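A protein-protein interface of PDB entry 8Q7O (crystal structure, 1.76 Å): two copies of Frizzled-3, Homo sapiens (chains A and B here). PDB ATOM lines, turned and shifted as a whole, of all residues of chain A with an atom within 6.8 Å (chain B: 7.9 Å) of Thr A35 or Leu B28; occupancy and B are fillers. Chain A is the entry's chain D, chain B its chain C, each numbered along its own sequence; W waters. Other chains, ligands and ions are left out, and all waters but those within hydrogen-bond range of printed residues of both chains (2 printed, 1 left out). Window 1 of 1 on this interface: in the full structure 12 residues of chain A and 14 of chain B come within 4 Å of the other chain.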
ATOM      1  N   ASN A  29      15.904  28.520 -23.216  1.00  0.00           N
ATOM      2  CA  ASN A  29      15.205  29.284 -22.183  1.00  0.00           C
ATOM      3  C   ASN A  29      13.747  28.871 -22.010  1.00  0.00           C
ATOM      4  O   ASN A  29      13.336  28.422 -20.931  1.00  0.00           O
ATOM      5  CB  ASN A  29      15.289  30.770 -22.529  1.00  0.00           C
ATOM      6  CG  ASN A  29      14.524  31.636 -21.559  1.00  0.00           C
ATOM      7  OD1 ASN A  29      14.545  31.415 -20.346  1.00  0.00           O
ATOM      8  ND2 ASN A  29      13.816  32.624 -22.095  1.00  0.00           N
ATOM      9  N   HIS A  30      12.932  29.071 -23.050  1.00  0.00           N
ATOM     10  CA  HIS A  30      11.509  28.773 -22.920  1.00  0.00           C
ATOM     11  C   HIS A  30      11.282  27.335 -22.481  1.00  0.00           C
ATOM     12  O   HIS A  30      10.463  27.071 -21.591  1.00  0.00           O
ATOM     13  CB  HIS A  30      10.767  29.110 -24.222  1.00  0.00           C
ATOM     14  CG  HIS A  30      10.700  30.585 -24.497  1.00  0.00           C
ATOM     15  ND1 HIS A  30      10.216  31.487 -23.568  1.00  0.00           N
ATOM     16  CD2 HIS A  30      11.049  31.316 -25.583  1.00  0.00           C
ATOM     17  CE1 HIS A  30      10.277  32.709 -24.070  1.00  0.00           C
ATOM     18  NE2 HIS A  30      10.782  32.634 -25.290  1.00  0.00           N
ATOM     19  N   TYR A  31      12.007  26.391 -23.078  1.00  0.00           N
ATOM     20  CA  TYR A  31      11.894  24.994 -22.673  1.00  0.00           C
ATOM     21  C   TYR A  31      12.272  24.775 -21.203  1.00  0.00           C
ATOM     22  O   TYR A  31      11.568  24.071 -20.465  1.00  0.00           O
ATOM     23  CB  TYR A  31      12.782  24.149 -23.579  1.00  0.00           C
ATOM     24  CG  TYR A  31      12.839  22.729 -23.149  1.00  0.00           C
ATOM     25  CD1 TYR A  31      11.687  21.949 -23.141  1.00  0.00           C
ATOM     26  CD2 TYR A  31      14.028  22.157 -22.745  1.00  0.00           C
ATOM     27  CE1 TYR A  31      11.722  20.638 -22.737  1.00  0.00           C
ATOM     28  CE2 TYR A  31      14.074  20.841 -22.338  1.00  0.00           C
ATOM     29  CZ  TYR A  31      12.918  20.090 -22.338  1.00  0.00           C
ATOM     30  OH  TYR A  31      12.946  18.775 -21.932  1.00  0.00           O
ATOM     31  N   ASP A  32      13.384  25.365 -20.764  1.00  0.00           N
ATOM     32  CA  ASP A  32      13.823  25.208 -19.378  1.00  0.00           C
ATOM     33  C   ASP A  32      12.812  25.801 -18.408  1.00  0.00           C
ATOM     34  O   ASP A  32      12.544  25.221 -17.349  1.00  0.00           O
ATOM     35  CB  ASP A  32      15.209  25.844 -19.185  1.00  0.00           C
ATOM     36  CG  ASP A  32      16.314  25.037 -19.841  1.00  0.00           C
ATOM     37  OD1 ASP A  32      16.006  23.951 -20.387  1.00  0.00           O
ATOM     38  OD2 ASP A  32      17.486  25.481 -19.827  1.00  0.00           O
ATOM     39  N   GLN A  33      12.287  26.990 -18.719  1.00  0.00           N
ATOM     40  CA  GLN A  33      11.327  27.616 -17.819  1.00  0.00           C
ATOM     41  C   GLN A  33       9.982  26.904 -17.842  1.00  0.00           C
ATOM     42  O   GLN A  33       9.283  26.877 -16.825  1.00  0.00           O
ATOM     43  CB  GLN A  33      11.176  29.100 -18.150  1.00  0.00           C
ATOM     44  CG  GLN A  33      12.443  29.915 -17.833  1.00  0.00           C
ATOM     45  CD  GLN A  33      12.126  31.362 -17.529  1.00  0.00           C
ATOM     46  OE1 GLN A  33      11.230  31.651 -16.730  1.00  0.00           O
ATOM     47  NE2 GLN A  33      12.844  32.288 -18.180  1.00  0.00           N
ATOM     48  N   GLN A  34       9.604  26.327 -18.983  1.00  0.00           N
ATOM     49  CA  GLN A  34       8.397  25.505 -19.028  1.00  0.00           C
ATOM     50  C   GLN A  34       8.549  24.278 -18.138  1.00  0.00           C
ATOM     51  O   GLN A  34       7.613  23.891 -17.416  1.00  0.00           O
ATOM     52  CB  GLN A  34       8.102  25.090 -20.464  1.00  0.00           C
ATOM     53  CG  GLN A  34       7.573  26.198 -21.327  1.00  0.00           C
ATOM     54  CD  GLN A  34       7.357  25.749 -22.761  1.00  0.00           C
ATOM     55  OE1 GLN A  34       6.655  24.765 -23.022  1.00  0.00           O
ATOM     56  NE2 GLN A  34       7.964  26.464 -23.696  1.00  0.00           N
ATOM     57  N   THR A  35       9.726  23.656 -18.176  1.00  0.00           N
ATOM     58  CA  THR A  35       9.984  22.499 -17.334  1.00  0.00           C
ATOM     59  C   THR A  35       9.975  22.883 -15.858  1.00  0.00           C
ATOM     60  O   THR A  35       9.375  22.178 -15.035  1.00  0.00           O
ATOM     61  CB  THR A  35      11.326  21.873 -17.723  1.00  0.00           C
ATOM     62  OG1 THR A  35      11.249  21.344 -19.063  1.00  0.00           O
ATOM     63  CG2 THR A  35      11.719  20.783 -16.741  1.00  0.00           C
ATOM     64  N   ALA A  36      10.582  24.028 -15.516  1.00  0.00           N
ATOM     65  CA  ALA A  36      10.565  24.493 -14.130  1.00  0.00           C
ATOM     66  C   ALA A  36       9.144  24.791 -13.664  1.00  0.00           C
ATOM     67  O   ALA A  36       8.769  24.445 -12.534  1.00  0.00           O
ATOM     68  CB  ALA A  36      11.455  25.730 -13.966  1.00  0.00           C
ATOM     69  N   ALA A  37       8.349  25.463 -14.505  1.00  0.00           N
ATOM     70  CA  ALA A  37       6.957  25.740 -14.152  1.00  0.00           C
ATOM     71  C   ALA A  37       6.181  24.455 -13.895  1.00  0.00           C
ATOM     72  O   ALA A  37       5.345  24.404 -12.984  1.00  0.00           O
ATOM     73  CB  ALA A  37       6.269  26.552 -15.251  1.00  0.00           C
ATOM     74  N   LEU A  38       6.415  23.421 -14.710  1.00  0.00           N
ATOM     75  CA  LEU A  38       5.746  22.137 -14.500  1.00  0.00           C
ATOM     76  C   LEU A  38       6.151  21.513 -13.173  1.00  0.00           C
ATOM     77  O   LEU A  38       5.311  20.935 -12.460  1.00  0.00           O
ATOM     78  CB  LEU A  38       6.081  21.172 -15.639  1.00  0.00           C
ATOM     79  CG  LEU A  38       5.163  19.952 -15.696  1.00  0.00           C
ATOM     80  CD1 LEU A  38       3.721  20.394 -15.779  1.00  0.00           C
ATOM     81  CD2 LEU A  38       5.561  19.037 -16.846  1.00  0.00           C
ATOM     82  N   ALA A  39       7.445  21.604 -12.840  1.00  0.00           N
ATOM     83  CA  ALA A  39       7.950  21.014 -11.608  1.00  0.00           C
ATOM     84  C   ALA A  39       7.402  21.733 -10.386  1.00  0.00           C
ATOM     85  O   ALA A  39       7.209  21.109  -9.337  1.00  0.00           O
ATOM     86  CB  ALA A  39       9.483  21.039 -11.598  1.00  0.00           C
ATOM     87  N   MET A  40       7.137  23.037 -10.511  1.00  0.00           N
ATOM     88  CA  MET A  40       6.670  23.851  -9.394  1.00  0.00           C
ATOM     89  C   MET A  40       5.161  23.768  -9.199  1.00  0.00           C
ATOM     90  O   MET A  40       4.671  24.041  -8.095  1.00  0.00           O
ATOM     91  CB  MET A  40       7.052  25.312  -9.615  1.00  0.00           C
ATOM     92  CG  MET A  40       6.919  26.178  -8.375  1.00  0.00           C
ATOM     93  SD  MET A  40       7.486  27.857  -8.690  1.00  0.00           S
ATOM     94  CE  MET A  40       6.827  28.655  -7.231  1.00  0.00           C
ATOM     95  N   TYR A  63      13.627  27.450  -8.343  1.00  0.00           N
ATOM     96  CA  TYR A  63      13.172  27.280  -9.719  1.00  0.00           C
ATOM     97  C   TYR A  63      13.460  28.483 -10.606  1.00  0.00           C
ATOM     98  O   TYR A  63      13.542  28.319 -11.830  1.00  0.00           O
ATOM     99  CB  TYR A  63      11.656  27.006  -9.747  1.00  0.00           C
ATOM    100  CG  TYR A  63      11.273  25.690  -9.119  1.00  0.00           C
ATOM    101  CD1 TYR A  63      11.631  24.494  -9.722  1.00  0.00           C
ATOM    102  CD2 TYR A  63      10.564  25.640  -7.919  1.00  0.00           C
ATOM    103  CE1 TYR A  63      11.297  23.269  -9.152  1.00  0.00           C
ATOM    104  CE2 TYR A  63      10.217  24.413  -7.337  1.00  0.00           C
ATOM    105  CZ  TYR A  63      10.585  23.236  -7.966  1.00  0.00           C
ATOM    106  OH  TYR A  63      10.258  22.013  -7.418  1.00  0.00           O
ATOM    107  N   ASP A 102      15.612  16.685  -2.912  1.00  0.00           N
ATOM    108  CA  ASP A 102      16.509  17.795  -3.224  1.00  0.00           C
ATOM    109  C   ASP A 102      16.094  19.097  -2.555  1.00  0.00           C
ATOM    110  O   ASP A 102      16.761  20.114  -2.769  1.00  0.00           O
ATOM    111  CB  ASP A 102      16.619  17.992  -4.743  1.00  0.00           C
ATOM    112  CG  ASP A 102      15.263  18.038  -5.445  1.00  0.00           C
ATOM    113  OD1 ASP A 102      14.230  18.305  -4.789  1.00  0.00           O
ATOM    114  OD2 ASP A 102      15.230  17.807  -6.674  1.00  0.00           O
ATOM    115  N   GLU B   7      22.170  10.457 -16.282  1.00  0.00           N
ATOM    116  CA  GLU B   7      21.137   9.443 -16.203  1.00  0.00           C
ATOM    117  C   GLU B   7      20.827   8.878 -17.594  1.00  0.00           C
ATOM    118  O   GLU B   7      21.019   9.563 -18.608  1.00  0.00           O
ATOM    119  CB  GLU B   7      19.860   9.991 -15.561  1.00  0.00           C
ATOM    120  CG  GLU B   7      19.072  10.962 -16.395  1.00  0.00           C
ATOM    121  CD  GLU B   7      17.797  11.374 -15.686  1.00  0.00           C
ATOM    122  OE1 GLU B   7      17.762  11.255 -14.438  1.00  0.00           O
ATOM    123  OE2 GLU B   7      16.844  11.804 -16.367  1.00  0.00           O
ATOM    124  N   MET B  24      20.582  15.671 -15.984  1.00  0.00           N
ATOM    125  CA  MET B  24      19.242  16.057 -15.553  1.00  0.00           C
ATOM    126  C   MET B  24      19.385  16.725 -14.195  1.00  0.00           C
ATOM    127  O   MET B  24      19.821  16.068 -13.228  1.00  0.00           O
ATOM    128  CB  MET B  24      18.327  14.835 -15.457  1.00  0.00           C
ATOM    129  CG  MET B  24      16.888  15.182 -15.131  1.00  0.00           C
ATOM    130  SD  MET B  24      16.100  16.064 -16.494  1.00  0.00           S
ATOM    131  CE  MET B  24      15.966  14.754 -17.712  1.00  0.00           C
ATOM    132  N   PRO B  25      18.999  17.991 -14.057  1.00  0.00           N
ATOM    133  CA  PRO B  25      18.951  18.604 -12.725  1.00  0.00           C
ATOM    134  C   PRO B  25      17.898  17.912 -11.875  1.00  0.00           C
ATOM    135  O   PRO B  25      16.816  17.581 -12.367  1.00  0.00           O
ATOM    136  CB  PRO B  25      18.581  20.068 -13.013  1.00  0.00           C
ATOM    137  CG  PRO B  25      18.751  20.246 -14.521  1.00  0.00           C
ATOM    138  CD  PRO B  25      18.499  18.897 -15.106  1.00  0.00           C
ATOM    139  N   ASN B  26      18.232  17.682 -10.595  1.00  0.00           N
ATOM    140  CA  ASN B  26      17.358  16.891  -9.725  1.00  0.00           C
ATOM    141  C   ASN B  26      15.956  17.472  -9.658  1.00  0.00           C
ATOM    142  O   ASN B  26      14.967  16.736  -9.767  1.00  0.00           O
ATOM    143  CB  ASN B  26      17.942  16.768  -8.316  1.00  0.00           C
ATOM    144  CG  ASN B  26      19.088  15.783  -8.243  1.00  0.00           C
ATOM    145  OD1 ASN B  26      19.210  14.896  -9.093  1.00  0.00           O
ATOM    146  ND2 ASN B  26      19.924  15.913  -7.214  1.00  0.00           N
ATOM    147  N   LEU B  27      15.848  18.792  -9.514  1.00  0.00           N
ATOM    148  CA  LEU B  27      14.540  19.411  -9.351  1.00  0.00           C
ATOM    149  C   LEU B  27      13.657  19.202 -10.570  1.00  0.00           C
ATOM    150  O   LEU B  27      12.427  19.248 -10.451  1.00  0.00           O
ATOM    151  CB  LEU B  27      14.707  20.910  -9.118  1.00  0.00           C
ATOM    152  CG  LEU B  27      15.092  21.391  -7.718  1.00  0.00           C
ATOM    153  CD1 LEU B  27      15.506  22.855  -7.807  1.00  0.00           C
ATOM    154  CD2 LEU B  27      13.965  21.202  -6.734  1.00  0.00           C
ATOM    155  N   LEU B  28      14.248  18.988 -11.742  1.00  0.00           N
ATOM    156  CA  LEU B  28      13.478  18.921 -12.973  1.00  0.00           C
ATOM    157  C   LEU B  28      13.255  17.506 -13.485  1.00  0.00           C
ATOM    158  O   LEU B  28      12.554  17.341 -14.479  1.00  0.00           O
ATOM    159  CB  LEU B  28      14.167  19.758 -14.057  1.00  0.00           C
ATOM    160  CG  LEU B  28      14.406  21.189 -13.572  1.00  0.00           C
ATOM    161  CD1 LEU B  28      15.221  21.994 -14.601  1.00  0.00           C
ATOM    162  CD2 LEU B  28      13.087  21.874 -13.228  1.00  0.00           C
ATOM    163  N   ASN B  29      13.836  16.486 -12.857  1.00  0.00           N
ATOM    164  CA  ASN B  29      13.684  15.137 -13.394  1.00  0.00           C
ATOM    165  C   ASN B  29      12.199  14.770 -13.480  1.00  0.00           C
ATOM    166  O   ASN B  29      11.394  15.196 -12.650  1.00  0.00           O
ATOM    167  CB  ASN B  29      14.439  14.119 -12.538  1.00  0.00           C
ATOM    168  CG  ASN B  29      14.413  12.731 -13.155  1.00  0.00           C
ATOM    169  OD1 ASN B  29      14.568  12.587 -14.375  1.00  0.00           O
ATOM    170  ND2 ASN B  29      14.197  11.708 -12.329  1.00  0.00           N
ATOM    171  N   HIS B  30      11.850  13.999 -14.521  1.00  0.00           N
ATOM    172  CA  HIS B  30      10.500  13.571 -14.886  1.00  0.00           C
ATOM    173  C   HIS B  30       9.740  14.719 -15.547  1.00  0.00           C
ATOM    174  O   HIS B  30       9.195  14.558 -16.643  1.00  0.00           O
ATOM    175  CB  HIS B  30       9.735  13.046 -13.666  1.00  0.00           C
ATOM    176  CG  HIS B  30      10.381  11.852 -13.036  1.00  0.00           C
ATOM    177  ND1 HIS B  30      10.696  10.712 -13.743  1.00  0.00           N
ATOM    178  CD2 HIS B  30      10.814  11.640 -11.769  1.00  0.00           C
ATOM    179  CE1 HIS B  30      11.277   9.841 -12.935  1.00  0.00           C
ATOM    180  NE2 HIS B  30      11.360  10.380 -11.731  1.00  0.00           N
ATOM    181  N   TYR B  31       9.729  15.890 -14.912  1.00  0.00           N
ATOM    182  CA  TYR B  31       9.083  17.050 -15.517  1.00  0.00           C
ATOM    183  C   TYR B  31       9.731  17.387 -16.848  1.00  0.00           C
ATOM    184  O   TYR B  31       9.043  17.727 -17.823  1.00  0.00           O
ATOM    185  CB  TYR B  31       9.144  18.231 -14.551  1.00  0.00           C
ATOM    186  CG  TYR B  31       8.519  17.853 -13.235  1.00  0.00           C
ATOM    187  CD1 TYR B  31       7.144  17.650 -13.146  1.00  0.00           C
ATOM    188  CD2 TYR B  31       9.297  17.627 -12.106  1.00  0.00           C
ATOM    189  CE1 TYR B  31       6.552  17.274 -11.945  1.00  0.00           C
ATOM    190  CE2 TYR B  31       8.711  17.248 -10.897  1.00  0.00           C
ATOM    191  CZ  TYR B  31       7.343  17.074 -10.833  1.00  0.00           C
ATOM    192  OH  TYR B  31       6.756  16.695  -9.637  1.00  0.00           O
ATOM    193  N   ASP B  32      11.059  17.281 -16.904  1.00  0.00           N
ATOM    194  CA  ASP B  32      11.780  17.568 -18.138  1.00  0.00           C
ATOM    195  C   ASP B  32      11.363  16.620 -19.257  1.00  0.00           C
ATOM    196  O   ASP B  32      11.072  17.056 -20.373  1.00  0.00           O
ATOM    197  CB  ASP B  32      13.277  17.478 -17.881  1.00  0.00           C
ATOM    198  CG  ASP B  32      14.090  17.778 -19.113  1.00  0.00           C
ATOM    199  OD1 ASP B  32      14.154  16.906 -20.010  1.00  0.00           O
ATOM    200  OD2 ASP B  32      14.642  18.904 -19.193  1.00  0.00           O
ATOM    201  N   GLN B  33      11.294  15.323 -18.968  1.00  0.00           N
ATOM    202  CA  GLN B  33      10.940  14.385 -20.025  1.00  0.00           C
ATOM    203  C   GLN B  33       9.495  14.563 -20.464  1.00  0.00           C
ATOM    204  O   GLN B  33       9.185  14.356 -21.644  1.00  0.00           O
ATOM    205  CB  GLN B  33      11.190  12.949 -19.572  1.00  0.00           C
ATOM    206  CG  GLN B  33      12.672  12.625 -19.359  1.00  0.00           C
ATOM    207  CD  GLN B  33      13.111  12.813 -17.914  1.00  0.00           C
ATOM    208  OE1 GLN B  33      12.689  13.755 -17.232  1.00  0.00           O
ATOM    209  NE2 GLN B  33      13.960  11.909 -17.435  1.00  0.00           N
ATOM    210  N   GLN B  34       8.616  14.982 -19.551  1.00  0.00           N
ATOM    211  CA  GLN B  34       7.237  15.276 -19.932  1.00  0.00           C
ATOM    212  C   GLN B  34       7.167  16.447 -20.902  1.00  0.00           C
ATOM    213  O   GLN B  34       6.456  16.391 -21.913  1.00  0.00           O
ATOM    214  CB  GLN B  34       6.402  15.597 -18.693  1.00  0.00           C
ATOM    215  CG  GLN B  34       6.095  14.432 -17.794  1.00  0.00           C
ATOM    216  CD  GLN B  34       5.291  14.876 -16.592  1.00  0.00           C
ATOM    217  OE1 GLN B  34       5.794  14.919 -15.471  1.00  0.00           O
ATOM    218  NE2 GLN B  34       4.026  15.224 -16.829  1.00  0.00           N
ATOM    219  N   THR B  35       7.900  17.524 -20.603  1.00  0.00           N
ATOM    220  CA  THR B  35       7.912  18.688 -21.484  1.00  0.00           C
ATOM    221  C   THR B  35       8.606  18.371 -22.804  1.00  0.00           C
ATOM    222  O   THR B  35       8.195  18.865 -23.860  1.00  0.00           O
ATOM    223  CB  THR B  35       8.587  19.864 -20.785  1.00  0.00           C
ATOM    224  OG1 THR B  35       9.922  19.484 -20.464  1.00  0.00           O
ATOM    225  CG2 THR B  35       7.850  20.218 -19.483  1.00  0.00           C
ATOM    226  N   ALA B  36       9.676  17.571 -22.755  1.00  0.00           N
ATOM    227  CA  ALA B  36      10.365  17.158 -23.973  1.00  0.00           C
ATOM    228  C   ALA B  36       9.464  16.298 -24.858  1.00  0.00           C
ATOM    229  O   ALA B  36       9.371  16.524 -26.067  1.00  0.00           O
ATOM    230  CB  ALA B  36      11.653  16.407 -23.626  1.00  0.00           C
ATOM    231  N   TYR B  63      16.644  18.014 -26.877  1.00  0.00           N
ATOM    232  CA  TYR B  63      15.849  17.457 -25.790  1.00  0.00           C
ATOM    233  C   TYR B  63      16.533  16.347 -25.006  1.00  0.00           C
ATOM    234  O   TYR B  63      16.084  16.031 -23.900  1.00  0.00           O
ATOM    235  CB  TYR B  63      14.491  17.008 -26.344  1.00  0.00           C
ATOM    236  CG  TYR B  63      13.749  18.227 -26.839  1.00  0.00           C
ATOM    237  CD1 TYR B  63      13.291  19.189 -25.943  1.00  0.00           C
ATOM    238  CD2 TYR B  63      13.557  18.450 -28.197  1.00  0.00           C
ATOM    239  CE1 TYR B  63      12.636  20.327 -26.384  1.00  0.00           C
ATOM    240  CE2 TYR B  63      12.903  19.587 -28.648  1.00  0.00           C
ATOM    241  CZ  TYR B  63      12.450  20.519 -27.738  1.00  0.00           C
ATOM    242  OH  TYR B  63      11.801  21.648 -28.180  1.00  0.00           O
HETATM  243  O   HOH W   1      14.587  21.863 -19.035  1.00  0.00           O
HETATM  244  O   HOH W   2      10.978  19.647  -8.370  1.00  0.00           O
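Of chain B, only Leu B28, Tyr B31, Asp B32 and Thr B35 come within 4 Å of Thr A35. Printed residues of chain A within 4 Å of Leu B28: Thr A35 (3.8 Å) and Ala A36 (3.7 Å). Of chain B, only Leu B28 comes within 4 Å of Ala A36. Of the printed residues of chain B, Tyr A31 touches Asp B32, Thr B35, Ala B36 and Tyr B63. Printed residues of chain A within 4 Å of Tyr B31: Thr A35, Leu A38 and Ala A39. Pro B25 touches none of the printed residues of chain A.
Tyr A31 touches Asp B32, but with the chains exchanged Asp A32 does not touch Tyr B31 (8.3 Å). Tyr A31 touches Thr B35, and with the chains exchanged Thr A35 touches Tyr B31. Tyr A31 touches Tyr B63, but with the chains exchanged Tyr A63 does not touch Tyr B31 (6.1 Å). Thr A35 touches Asp B32, but with the chains exchanged Asp A32 does not touch Thr B35 (6.8 Å). Positions printed for both chains: 29, 30, 31, 32, 33, 34, 35, 36 and 63. Of the 17 pairs that touch across the chains among the printed residues, 3 have their exchanged pair printed and touching as well.
Printed residues of chain B that touch a printed residue of chain A: Asn B26, Leu B27, Leu B28, Tyr B31, Asp B32, Gln B34, Thr B35, Ala B36 and Tyr B63. Hydrophobic or aromatic side chains of chain B within 4 Å of the printed part of chain A: Leu B27, Leu B28, Tyr B31, Ala B36 and Tyr B63. Of the 14 printed residues of chain A, 7 touch a printed residue of chain B. Hydrophobic or aromatic side chains of chain A within 4 Å of the printed part of chain B: Tyr A31, Leu A38, Ala A39 and Tyr A63. Along chain A the printed residues that touch a printed residue of chain B span positions 31 to 102. Among the printed residues, no Asp or Glu carboxylate lies within 4 Å of a Lys or Arg side-chain nitrogen of the other chain.
The backbone carbonyl oxygen of Tyr B31 lies close to the side-chain hydroxyl of Thr B35. The backbone carbonyl oxygen of Asp B32 sits at hydrogen-bond distance from the side-chain hydroxyl of Thr B35, 2.7 Å away. The backbone carbonyl oxygen of Tyr A31 is in hydrogen-bond range of the side-chain hydroxyl of Thr A35.
Water W2 bridges O of Leu B27 and OH of Tyr A63. Water W1 lies within hydrogen-bond range of OD1 of Asp A32 (2.9 Å), OD2 of Asp B32 (3.0 Å) and OG1 of Thr A35 (3.4 Å).
Among the printed residues, pairs that only touch across the chains: Tyr A31 with Ala B36 (3.2 Å), Tyr A31 with Tyr B63 (3.7 Å), Thr A35 with Leu B28 (3.8 Å), Thr A35 with Tyr B31 (3.9 Å), Thr A35 with Asp B32 (3.5 Å), Ala A36 with Leu B28 (3.7 Å), Leu A38 with Tyr B31 (3.8 Å), Leu A38 with Gln B34 (3.99 Å), Leu A38 with Thr B35 (3.7 Å), Ala A39 with Leu B27 (3.6 Å), Ala A39 with Tyr B31 (3.5 Å) and Tyr A63 with Leu B27 (3.9 Å).
The side-chain carboxylate of Asp A102 is in hydrogen-bond range of the backbone NH of Leu B27, at 3.1 Å. The side-chain carboxylate (OD1) of Asp B32 is in hydrogen-bond range of the side-chain hydroxyl (OH) of Tyr A31, at 2.9 Å. OH of Tyr A31 sits close to OG1 of Thr B35, 3.4 Å away. The side-chain hydroxyl (OG1) of Thr B35 lies within hydrogen-bond range of the side-chain hydroxyl (OG1) of Thr A35 (2.7 Å). The side-chain carboxylate of Asp A102 lies close to the backbone carbonyl oxygen of Asn B26 (3.3 Å).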
